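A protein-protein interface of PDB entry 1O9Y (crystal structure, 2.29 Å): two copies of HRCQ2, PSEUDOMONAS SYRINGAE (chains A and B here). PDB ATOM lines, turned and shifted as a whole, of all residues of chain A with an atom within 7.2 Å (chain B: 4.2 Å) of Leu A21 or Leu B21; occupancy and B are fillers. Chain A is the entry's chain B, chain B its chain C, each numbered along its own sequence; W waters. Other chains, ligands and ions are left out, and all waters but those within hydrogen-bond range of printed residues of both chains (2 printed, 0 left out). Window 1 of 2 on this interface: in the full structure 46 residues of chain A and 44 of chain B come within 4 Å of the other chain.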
ATOM      1  N   LEU A  19      -0.674  18.792  33.806  1.00  0.00           N
ATOM      2  CA  LEU A  19      -0.973  18.385  32.449  1.00  0.00           C
ATOM      3  C   LEU A  19      -1.155  16.878  32.380  1.00  0.00           C
ATOM      4  O   LEU A  19      -0.623  16.142  33.206  1.00  0.00           O
ATOM      5  CB  LEU A  19       0.118  18.858  31.477  1.00  0.00           C
ATOM      6  CG  LEU A  19       0.517  20.340  31.463  1.00  0.00           C
ATOM      7  CD1 LEU A  19       1.846  20.537  30.777  1.00  0.00           C
ATOM      8  CD2 LEU A  19      -0.524  21.217  30.802  1.00  0.00           C
ATOM      9  N   THR A  20      -1.934  16.431  31.403  1.00  0.00           N
ATOM     10  CA  THR A  20      -2.165  15.011  31.190  1.00  0.00           C
ATOM     11  C   THR A  20      -1.848  14.634  29.747  1.00  0.00           C
ATOM     12  O   THR A  20      -1.909  15.462  28.838  1.00  0.00           O
ATOM     13  CB  THR A  20      -3.635  14.633  31.490  1.00  0.00           C
ATOM     14  OG1 THR A  20      -4.486  15.288  30.549  1.00  0.00           O
ATOM     15  CG2 THR A  20      -4.106  15.176  32.847  1.00  0.00           C
ATOM     16  N   LEU A  21      -1.525  13.367  29.558  1.00  0.00           N
ATOM     17  CA  LEU A  21      -1.300  12.821  28.235  1.00  0.00           C
ATOM     18  C   LEU A  21      -2.565  12.101  27.774  1.00  0.00           C
ATOM     19  O   LEU A  21      -3.011  11.125  28.389  1.00  0.00           O
ATOM     20  CB  LEU A  21      -0.069  11.896  28.240  1.00  0.00           C
ATOM     21  CG  LEU A  21       1.316  12.570  28.264  1.00  0.00           C
ATOM     22  CD1 LEU A  21       1.648  13.238  29.615  1.00  0.00           C
ATOM     23  CD2 LEU A  21       2.396  11.563  27.897  1.00  0.00           C
ATOM     24  N   ARG A  22      -3.164  12.629  26.713  1.00  0.00           N
ATOM     25  CA  ARG A  22      -4.321  12.019  26.091  1.00  0.00           C
ATOM     26  C   ARG A  22      -3.780  11.181  24.943  1.00  0.00           C
ATOM     27  O   ARG A  22      -3.169  11.723  24.014  1.00  0.00           O
ATOM     28  CB  ARG A  22      -5.282  13.108  25.609  1.00  0.00           C
ATOM     29  CG  ARG A  22      -6.572  12.626  24.963  1.00  0.00           C
ATOM     30  CD  ARG A  22      -7.530  13.745  24.560  1.00  0.00           C
ATOM     31  NE  ARG A  22      -7.231  14.291  23.228  1.00  0.00           N
ATOM     32  CZ  ARG A  22      -7.282  15.589  22.908  1.00  0.00           C
ATOM     33  N   CYS A  23      -3.970   9.856  25.023  1.00  0.00           N
ATOM     34  CA  CYS A  23      -3.464   8.945  23.992  1.00  0.00           C
ATOM     35  C   CYS A  23      -4.584   8.174  23.301  1.00  0.00           C
ATOM     36  O   CYS A  23      -4.407   7.016  22.895  1.00  0.00           O
ATOM     37  CB  CYS A  23      -2.411   7.989  24.560  1.00  0.00           C
ATOM     38  SG  CYS A  23      -2.883   7.160  26.105  1.00  0.00           S
ATOM     39  N   GLY A  24      -5.734   8.828  23.162  1.00  0.00           N
ATOM     40  CA  GLY A  24      -6.872   8.230  22.502  1.00  0.00           C
ATOM     41  C   GLY A  24      -8.170   8.677  23.125  1.00  0.00           C
ATOM     42  O   GLY A  24      -8.196   9.079  24.275  1.00  0.00           O
ATOM     43  N   GLU A  25      -9.235   8.616  22.340  1.00  0.00           N
ATOM     44  CA  GLU A  25     -10.585   8.962  22.780  1.00  0.00           C
ATOM     45  C   GLU A  25     -11.586   7.936  22.262  1.00  0.00           C
ATOM     46  O   GLU A  25     -11.460   7.440  21.137  1.00  0.00           O
ATOM     47  CB  GLU A  25     -10.973  10.368  22.292  1.00  0.00           C
ATOM     48  CG  GLU A  25     -10.140  11.487  22.915  1.00  0.00           C
ATOM     49  CD  GLU A  25     -10.664  12.877  22.605  1.00  0.00           C
ATOM     50  OE1 GLU A  25     -10.145  13.497  21.642  1.00  0.00           O
ATOM     51  OE2 GLU A  25     -11.583  13.349  23.323  1.00  0.00           O
ATOM     52  N   LEU A  26     -12.572   7.606  23.088  1.00  0.00           N
ATOM     53  CA  LEU A  26     -13.655   6.723  22.661  1.00  0.00           C
ATOM     54  C   LEU A  26     -14.961   7.007  23.387  1.00  0.00           C
ATOM     55  O   LEU A  26     -14.983   7.664  24.431  1.00  0.00           O
ATOM     56  CB  LEU A  26     -13.265   5.246  22.789  1.00  0.00           C
ATOM     57  CG  LEU A  26     -13.181   4.568  24.153  1.00  0.00           C
ATOM     58  CD1 LEU A  26     -13.942   3.275  24.077  1.00  0.00           C
ATOM     59  CD2 LEU A  26     -11.753   4.283  24.472  1.00  0.00           C
ATOM     60  N   LEU A  42     -10.438  -3.038  23.896  1.00  0.00           N
ATOM     61  CA  LEU A  42     -11.156  -1.930  23.292  1.00  0.00           C
ATOM     62  C   LEU A  42     -10.300  -1.323  22.185  1.00  0.00           C
ATOM     63  O   LEU A  42      -9.114  -1.034  22.387  1.00  0.00           O
ATOM     64  CB  LEU A  42     -11.456  -0.857  24.331  1.00  0.00           C
ATOM     65  CG  LEU A  42     -12.406  -1.186  25.474  1.00  0.00           C
ATOM     66  CD1 LEU A  42     -12.578   0.071  26.325  1.00  0.00           C
ATOM     67  CD2 LEU A  42     -13.754  -1.696  24.988  1.00  0.00           C
ATOM     68  N   VAL A  44      -9.297   1.647  19.681  1.00  0.00           N
ATOM     69  CA  VAL A  44      -9.291   3.096  19.891  1.00  0.00           C
ATOM     70  C   VAL A  44      -8.857   3.733  18.582  1.00  0.00           C
ATOM     71  O   VAL A  44      -7.664   3.968  18.355  1.00  0.00           O
ATOM     72  CB  VAL A  44      -8.361   3.500  21.071  1.00  0.00           C
ATOM     73  CG1 VAL A  44      -8.384   5.013  21.312  1.00  0.00           C
ATOM     74  CG2 VAL A  44      -8.780   2.778  22.350  1.00  0.00           C
ATOM     75  N   ILE A  47      -6.311   7.565  16.203  1.00  0.00           N
ATOM     76  CA  ILE A  47      -5.000   7.915  16.730  1.00  0.00           C
ATOM     77  C   ILE A  47      -3.955   6.892  16.265  1.00  0.00           C
ATOM     78  O   ILE A  47      -4.221   5.686  16.225  1.00  0.00           O
ATOM     79  CB  ILE A  47      -5.044   8.001  18.276  1.00  0.00           C
ATOM     80  CG1 ILE A  47      -3.785   8.693  18.822  1.00  0.00           C
ATOM     81  CG2 ILE A  47      -5.269   6.600  18.909  1.00  0.00           C
ATOM     82  CD1 ILE A  47      -4.051   9.618  19.998  1.00  0.00           C
ATOM     83  N   HIS A  51       1.194   7.961  19.847  1.00  0.00           N
ATOM     84  CA  HIS A  51       0.940   9.394  19.835  1.00  0.00           C
ATOM     85  C   HIS A  51       0.188   9.797  21.098  1.00  0.00           C
ATOM     86  O   HIS A  51      -0.643   9.039  21.607  1.00  0.00           O
ATOM     87  CB  HIS A  51       0.136   9.805  18.606  1.00  0.00           C
ATOM     88  CG  HIS A  51       0.165  11.275  18.344  1.00  0.00           C
ATOM     89  ND1 HIS A  51       1.231  11.898  17.732  1.00  0.00           N
ATOM     90  CD2 HIS A  51      -0.729  12.252  18.637  1.00  0.00           C
ATOM     91  CE1 HIS A  51       0.984  13.194  17.640  1.00  0.00           C
ATOM     92  NE2 HIS A  51      -0.202  13.433  18.173  1.00  0.00           N
ATOM     93  N   ALA A  52       0.499  10.988  21.602  1.00  0.00           N
ATOM     94  CA  ALA A  52      -0.201  11.554  22.749  1.00  0.00           C
ATOM     95  C   ALA A  52      -0.314  13.053  22.555  1.00  0.00           C
ATOM     96  O   ALA A  52       0.573  13.676  21.966  1.00  0.00           O
ATOM     97  CB  ALA A  52       0.546  11.229  24.073  1.00  0.00           C
ATOM     98  N   THR A  53      -1.407  13.632  23.035  1.00  0.00           N
ATOM     99  CA  THR A  53      -1.481  15.085  23.134  1.00  0.00           C
ATOM    100  C   THR A  53      -1.316  15.430  24.600  1.00  0.00           C
ATOM    101  O   THR A  53      -1.784  14.692  25.490  1.00  0.00           O
ATOM    102  CB  THR A  53      -2.805  15.666  22.557  1.00  0.00           C
ATOM    103  OG1 THR A  53      -3.919  15.029  23.188  1.00  0.00           O
ATOM    104  CG2 THR A  53      -2.982  15.276  21.089  1.00  0.00           C
ATOM    105  N   LEU A  54      -0.609  16.526  24.839  1.00  0.00           N
ATOM    106  CA  LEU A  54      -0.406  17.038  26.172  1.00  0.00           C
ATOM    107  C   LEU A  54      -1.515  18.051  26.416  1.00  0.00           C
ATOM    108  O   LEU A  54      -1.687  18.994  25.648  1.00  0.00           O
ATOM    109  CB  LEU A  54       0.992  17.663  26.288  1.00  0.00           C
ATOM    110  CG  LEU A  54       1.495  18.162  27.634  1.00  0.00           C
ATOM    111  CD1 LEU A  54       1.811  16.993  28.540  1.00  0.00           C
ATOM    112  CD2 LEU A  54       2.734  18.988  27.413  1.00  0.00           C
ATOM    113  N   CYS A  55      -2.278  17.837  27.480  1.00  0.00           N
ATOM    114  CA  CYS A  55      -3.477  18.620  27.738  1.00  0.00           C
ATOM    115  C   CYS A  55      -3.502  19.288  29.095  1.00  0.00           C
ATOM    116  O   CYS A  55      -3.028  18.746  30.089  1.00  0.00           O
ATOM    117  CB  CYS A  55      -4.722  17.748  27.598  1.00  0.00           C
ATOM    118  SG  CYS A  55      -4.917  16.954  25.988  1.00  0.00           S
ATOM    119  N   GLU A  65       5.205  12.085  20.866  1.00  0.00           N
ATOM    120  CA  GLU A  65       5.218  10.621  20.831  1.00  0.00           C
ATOM    121  C   GLU A  65       5.633  10.077  22.191  1.00  0.00           C
ATOM    122  O   GLU A  65       6.513  10.638  22.838  1.00  0.00           O
ATOM    123  CB  GLU A  65       6.180  10.102  19.753  1.00  0.00           C
ATOM    124  CG  GLU A  65       5.858  10.529  18.322  1.00  0.00           C
ATOM    125  CD  GLU A  65       4.448  10.172  17.866  1.00  0.00           C
ATOM    126  OE1 GLU A  65       3.996   9.023  18.075  1.00  0.00           O
ATOM    127  OE2 GLU A  65       3.783  11.055  17.287  1.00  0.00           O
ATOM    128  N   LEU A  66       5.003   8.984  22.615  1.00  0.00           N
ATOM    129  CA  LEU A  66       5.387   8.296  23.845  1.00  0.00           C
ATOM    130  C   LEU A  66       6.695   7.551  23.634  1.00  0.00           C
ATOM    131  O   LEU A  66       6.813   6.727  22.728  1.00  0.00           O
ATOM    132  CB  LEU A  66       4.299   7.314  24.303  1.00  0.00           C
ATOM    133  CG  LEU A  66       2.909   7.818  24.737  1.00  0.00           C
ATOM    134  CD1 LEU A  66       2.039   6.646  25.181  1.00  0.00           C
ATOM    135  CD2 LEU A  66       2.986   8.853  25.833  1.00  0.00           C
ATOM    136  N   LEU A  73       8.877   6.195  31.101  1.00  0.00           N
ATOM    137  CA  LEU A  73       8.031   6.823  30.102  1.00  0.00           C
ATOM    138  C   LEU A  73       8.376   8.298  29.917  1.00  0.00           C
ATOM    139  O   LEU A  73       8.516   9.048  30.888  1.00  0.00           O
ATOM    140  CB  LEU A  73       6.545   6.645  30.437  1.00  0.00           C
ATOM    141  CG  LEU A  73       5.512   7.110  29.393  1.00  0.00           C
ATOM    142  CD1 LEU A  73       5.638   6.343  28.059  1.00  0.00           C
ATOM    143  CD2 LEU A  73       4.099   7.014  29.948  1.00  0.00           C
ATOM    144  N   GLY A  74       8.502   8.687  28.653  1.00  0.00           N
ATOM    145  CA  GLY A  74       8.741  10.060  28.265  1.00  0.00           C
ATOM    146  C   GLY A  74       7.756  10.468  27.181  1.00  0.00           C
ATOM    147  O   GLY A  74       7.124   9.612  26.542  1.00  0.00           O
ATOM    148  N   LEU A  75       7.605  11.774  26.994  1.00  0.00           N
ATOM    149  CA  LEU A  75       6.855  12.308  25.864  1.00  0.00           C
ATOM    150  C   LEU A  75       7.808  13.171  25.046  1.00  0.00           C
ATOM    151  O   LEU A  75       8.265  14.207  25.519  1.00  0.00           O
ATOM    152  CB  LEU A  75       5.633  13.136  26.335  1.00  0.00           C
ATOM    153  CG  LEU A  75       4.863  13.829  25.195  1.00  0.00           C
ATOM    154  CD1 LEU A  75       4.114  12.813  24.342  1.00  0.00           C
ATOM    155  CD2 LEU A  75       3.920  14.913  25.707  1.00  0.00           C
ATOM    156  N   GLN A  76       8.143  12.720  23.843  1.00  0.00           N
ATOM    157  CA  GLN A  76       8.985  13.502  22.945  1.00  0.00           C
ATOM    158  C   GLN A  76       8.089  14.468  22.178  1.00  0.00           C
ATOM    159  O   GLN A  76       7.237  14.038  21.402  1.00  0.00           O
ATOM    160  CB  GLN A  76       9.755  12.604  21.976  1.00  0.00           C
ATOM    161  CG  GLN A  76      10.559  13.388  20.915  1.00  0.00           C
ATOM    162  CD  GLN A  76      11.890  12.740  20.552  1.00  0.00           C
ATOM    163  OE1 GLN A  76      12.949  13.301  20.829  1.00  0.00           O
ATOM    164  NE2 GLN A  76      11.839  11.572  19.925  1.00  0.00           N
ATOM    165  N   THR B  20     -11.548   8.988  27.746  1.00  0.00           N
ATOM    166  CA  THR B  20     -10.223   9.323  27.282  1.00  0.00           C
ATOM    167  C   THR B  20      -9.212   8.243  27.706  1.00  0.00           C
ATOM    168  O   THR B  20      -9.294   7.731  28.822  1.00  0.00           O
ATOM    169  CB  THR B  20      -9.847  10.708  27.868  1.00  0.00           C
ATOM    170  OG1 THR B  20     -10.645  11.728  27.228  1.00  0.00           O
ATOM    171  CG2 THR B  20      -8.441  11.088  27.490  1.00  0.00           C
ATOM    172  N   LEU B  21      -8.277   7.900  26.816  1.00  0.00           N
ATOM    173  CA  LEU B  21      -7.103   7.136  27.223  1.00  0.00           C
ATOM    174  C   LEU B  21      -6.094   8.096  27.794  1.00  0.00           C
ATOM    175  O   LEU B  21      -5.762   9.097  27.166  1.00  0.00           O
ATOM    176  CB  LEU B  21      -6.491   6.362  26.059  1.00  0.00           C
ATOM    177  CG  LEU B  21      -6.823   4.877  25.999  1.00  0.00           C
ATOM    178  CD1 LEU B  21      -8.326   4.696  25.948  1.00  0.00           C
ATOM    179  CD2 LEU B  21      -6.145   4.201  24.798  1.00  0.00           C
ATOM    180  N   ARG B  22      -5.635   7.807  29.003  1.00  0.00           N
ATOM    181  CA  ARG B  22      -4.672   8.659  29.692  1.00  0.00           C
ATOM    182  C   ARG B  22      -3.363   7.905  29.886  1.00  0.00           C
ATOM    183  O   ARG B  22      -3.337   6.836  30.496  1.00  0.00           O
ATOM    184  CB  ARG B  22      -5.230   9.116  31.039  1.00  0.00           C
ATOM    185  CG  ARG B  22      -4.696  10.448  31.531  1.00  0.00           C
ATOM    186  CD  ARG B  22      -5.718  11.286  32.330  1.00  0.00           C
ATOM    187  NE  ARG B  22      -6.649  12.028  31.478  1.00  0.00           N
ATOM    188  CZ  ARG B  22      -7.420  13.024  31.909  1.00  0.00           C
ATOM    189  N   CYS B  23      -2.286   8.483  29.367  1.00  0.00           N
ATOM    190  CA  CYS B  23      -0.976   7.851  29.358  1.00  0.00           C
ATOM    191  C   CYS B  23       0.004   8.515  30.306  1.00  0.00           C
ATOM    192  O   CYS B  23       1.217   8.494  30.086  1.00  0.00           O
ATOM    193  CB  CYS B  23      -0.421   7.866  27.943  1.00  0.00           C
ATOM    194  SG  CYS B  23      -1.160   6.530  27.005  1.00  0.00           S
ATOM    195  N   GLY B  24      -0.536   9.106  31.361  1.00  0.00           N
ATOM    196  CA  GLY B  24       0.265   9.700  32.395  1.00  0.00           C
ATOM    197  C   GLY B  24       0.085  11.189  32.466  1.00  0.00           C
ATOM    198  O   GLY B  24      -0.758  11.779  31.792  1.00  0.00           O
ATOM    199  N   GLU B  25       0.919  11.799  33.295  1.00  0.00           N
ATOM    200  CA  GLU B  25       0.792  13.210  33.605  1.00  0.00           C
ATOM    201  C   GLU B  25       2.137  13.825  33.934  1.00  0.00           C
ATOM    202  O   GLU B  25       3.115  13.111  34.210  1.00  0.00           O
ATOM    203  CB  GLU B  25      -0.184  13.411  34.765  1.00  0.00           C
ATOM    204  CG  GLU B  25      -0.113  12.351  35.844  1.00  0.00           C
ATOM    205  CD  GLU B  25      -1.029  12.658  37.008  1.00  0.00           C
ATOM    206  OE1 GLU B  25      -0.505  13.056  38.076  1.00  0.00           O
ATOM    207  OE2 GLU B  25      -2.267  12.501  36.851  1.00  0.00           O
ATOM    208  N   LEU B  26       2.178  15.153  33.903  1.00  0.00           N
ATOM    209  CA  LEU B  26       3.372  15.903  34.274  1.00  0.00           C
ATOM    210  C   LEU B  26       3.007  17.345  34.603  1.00  0.00           C
ATOM    211  O   LEU B  26       1.960  17.852  34.187  1.00  0.00           O
ATOM    212  CB  LEU B  26       4.431  15.850  33.157  1.00  0.00           C
ATOM    213  CG  LEU B  26       4.049  16.354  31.763  1.00  0.00           C
ATOM    214  CD1 LEU B  26       4.517  17.806  31.568  1.00  0.00           C
ATOM    215  CD2 LEU B  26       4.635  15.453  30.701  1.00  0.00           C
ATOM    216  N   VAL B  44       7.343  11.516  32.300  1.00  0.00           N
ATOM    217  CA  VAL B  44       5.946  11.283  32.623  1.00  0.00           C
ATOM    218  C   VAL B  44       5.789  10.526  33.946  1.00  0.00           C
ATOM    219  O   VAL B  44       6.522   9.582  34.225  1.00  0.00           O
ATOM    220  CB  VAL B  44       5.228  10.496  31.482  1.00  0.00           C
ATOM    221  CG1 VAL B  44       3.743  10.360  31.762  1.00  0.00           C
ATOM    222  CG2 VAL B  44       5.474  11.158  30.121  1.00  0.00           C
ATOM    223  N   THR B  53      -4.775   4.512  31.551  1.00  0.00           N
ATOM    224  CA  THR B  53      -6.071   4.465  32.220  1.00  0.00           C
ATOM    225  C   THR B  53      -7.182   4.915  31.278  1.00  0.00           C
ATOM    226  O   THR B  53      -6.993   5.784  30.409  1.00  0.00           O
ATOM    227  CB  THR B  53      -6.116   5.321  33.520  1.00  0.00           C
ATOM    228  OG1 THR B  53      -5.627   6.648  33.261  1.00  0.00           O
ATOM    229  CG2 THR B  53      -5.179   4.771  34.586  1.00  0.00           C
ATOM    230  N   LEU B  54      -8.343   4.306  31.457  1.00  0.00           N
ATOM    231  CA  LEU B  54      -9.548   4.764  30.786  1.00  0.00           C
ATOM    232  C   LEU B  54     -10.228   5.765  31.711  1.00  0.00           C
ATOM    233  O   LEU B  54     -10.490   5.459  32.867  1.00  0.00           O
ATOM    234  CB  LEU B  54     -10.455   3.579  30.498  1.00  0.00           C
ATOM    235  CG  LEU B  54     -11.634   3.786  29.558  1.00  0.00           C
ATOM    236  CD1 LEU B  54     -11.171   4.310  28.207  1.00  0.00           C
ATOM    237  CD2 LEU B  54     -12.397   2.477  29.408  1.00  0.00           C
ATOM    238  N   LEU B  66      -1.665  -0.840  26.548  1.00  0.00           N
ATOM    239  CA  LEU B  66      -1.719  -0.432  25.147  1.00  0.00           C
ATOM    240  C   LEU B  66      -1.243  -1.562  24.226  1.00  0.00           C
ATOM    241  O   LEU B  66      -0.151  -2.091  24.393  1.00  0.00           O
ATOM    242  CB  LEU B  66      -0.912   0.858  24.915  1.00  0.00           C
ATOM    243  CG  LEU B  66      -1.297   2.083  25.756  1.00  0.00           C
ATOM    244  CD1 LEU B  66      -0.246   3.179  25.608  1.00  0.00           C
ATOM    245  CD2 LEU B  66      -2.658   2.605  25.376  1.00  0.00           C
ATOM    246  N   LEU B  73      -4.705   1.450  17.577  1.00  0.00           N
ATOM    247  CA  LEU B  73      -4.494   1.365  19.007  1.00  0.00           C
ATOM    248  C   LEU B  73      -5.619   0.562  19.674  1.00  0.00           C
ATOM    249  O   LEU B  73      -6.797   0.752  19.373  1.00  0.00           O
ATOM    250  CB  LEU B  73      -4.397   2.757  19.614  1.00  0.00           C
ATOM    251  CG  LEU B  73      -4.025   2.873  21.099  1.00  0.00           C
ATOM    252  CD1 LEU B  73      -2.649   2.261  21.441  1.00  0.00           C
ATOM    253  CD2 LEU B  73      -4.075   4.345  21.491  1.00  0.00           C
HETATM  254  O   HOH W   1      -6.035   3.918  16.306  1.00  0.00           O
HETATM  255  O   HOH W   2       9.120   8.456  34.018  1.00  0.00           O
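The backbone NH (N) of Leu A19 lies within hydrogen-bond range of the backbone carbonyl oxygen (O) of Leu B26 (2.8 Å).
The backbone NH (N) of Cys B23 sits at hydrogen-bond distance from the backbone carbonyl oxygen (O) of Leu A21.
O of Gly B24 is in hydrogen-bond range of N of Leu A21, 2.8 Å away.
N of Cys A23 lies within hydrogen-bond range of O of Leu B21 (2.9 Å).
The side-chain sulfur (SG) of Cys A23 forms a disulfide with the side-chain sulfur (SG) of Cys B23, at 2.0 Å.
The backbone carbonyl oxygen of Gly A24 lies within hydrogen-bond range of the backbone NH of Leu B21.
The backbone NH (N) of Val A44 is in hydrogen-bond range of the backbone carbonyl oxygen (O) of Leu B73.
The backbone carbonyl oxygen (O) of Leu A73 lies within hydrogen-bond range of the backbone NH (N) of Val B44 (3.1 Å).
Of the printed residues of chain B, Leu A21 touches Leu B21 (3.6 Å), Arg B22 (3.2 Å), Cys B23 (2.9 Å), Gly B24 (2.8 Å), Leu B26 (3.9 Å) and Val B44 (3.8 Å).
Leu B21 touches just these residues of chain A: Leu A21 (3.6 Å), Arg A22 (3.4 Å), Cys A23 (2.9 Å), Gly A24 (2.8 Å), Leu A26 (3.8 Å) and Val A44 (3.9 Å).
Of the printed residues of chain B, Leu A73 touches Cys B23 (3.2 Å) and Val B44 (3.1 Å).
Of the printed residues of chain A, Val B44 touches Leu A21, Leu A73, Gly A74 and Leu A75.
The nearest residue of chain A that does not touch Leu B21 is Glu A25 (4.6 Å).
Water W1 lies within hydrogen-bond range of O of Ile A47 (2.5 Å), O of Val A44 (2.6 Å) and N of Leu B73 (3.1 Å).
Water W2 lies within hydrogen-bond range of the backbone carbonyl oxygen (O) of Val B44 (2.8 Å) and the backbone carbonyl oxygen (O) of Leu A73 (3.2 Å).
Among the printed residues, merely in contact across the chains: Cys A23 with Leu B73 (3.0 Å), Leu A19 with Glu B25 (3.2 Å), Leu A73 with Cys B23 (3.2 Å), Leu A21 with Arg B22 (3.2 Å), Arg A22 with Leu B21 (3.4 Å), Arg A22 with Thr B20 (3.5 Å), Thr A20 with Gly B24 (3.6 Å), Leu A21 with Leu B21 (3.6 Å), Ile A47 with Leu B73 (3.6 Å), Gly A24 with Thr B20 (3.6 Å), Leu A66 with Cys B23 (3.7 Å), Leu A26 with Leu B21 (3.8 Å), Leu A26 with Leu B54 (3.8 Å), Gly A74 with Val B44 (3.8 Å), Leu A21 with Val B44 (3.8 Å), Leu A75 with Val B44 (3.8 Å), Val A44 with Leu B21 (3.9 Å), Leu A21 with Leu B26 (3.9 Å), Leu A54 with Leu B26 (3.9 Å), Cys A23 with Arg B22 (3.9 Å), Leu A42 with Leu B54 (3.9 Å) and Thr A20 with Arg B22 (3.9 Å).
Thr A20 touches Arg B22, and with the chains exchanged Arg A22 touches Thr B20.
Thr A20 touches Gly B24, and with the chains exchanged Gly A24 touches Thr B20.
Cys A23 touches Arg B22, but with the chains exchanged Arg A22 does not touch Cys B23 (5.0 Å).
Leu A66 touches Cys B23, but with the chains exchanged Cys A23 does not touch Leu B66 (4.6 Å).
Of the 12 printed residues of chain B, 10 touch a printed residue of chain A.
Hydrophobic or aromatic side chains of chain B that line the printed part of chain A: Leu B21, Leu B26, Val B44, Leu B54 and Leu B73.
Along chain A the printed residues that touch a printed residue of chain B span positions 19 to 75.
Among the printed residues, no Asp or Glu carboxylate lies within 4 Å of a Lys or Arg side-chain nitrogen of the other chain.
The backbone carbonyl oxygen (O) of Thr A20 sits at hydrogen-bond distance from the backbone NH (N) of Cys A55.
NE of Arg A22 lies within salt-bridge range of OE1 of Glu A25.
The backbone NH (N) of Arg A22 lies within hydrogen-bond range of the backbone carbonyl oxygen (O) of Thr A53 (2.8 Å).
N of Arg B22 is in hydrogen-bond range of O of Thr B53, at 2.8 Å.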
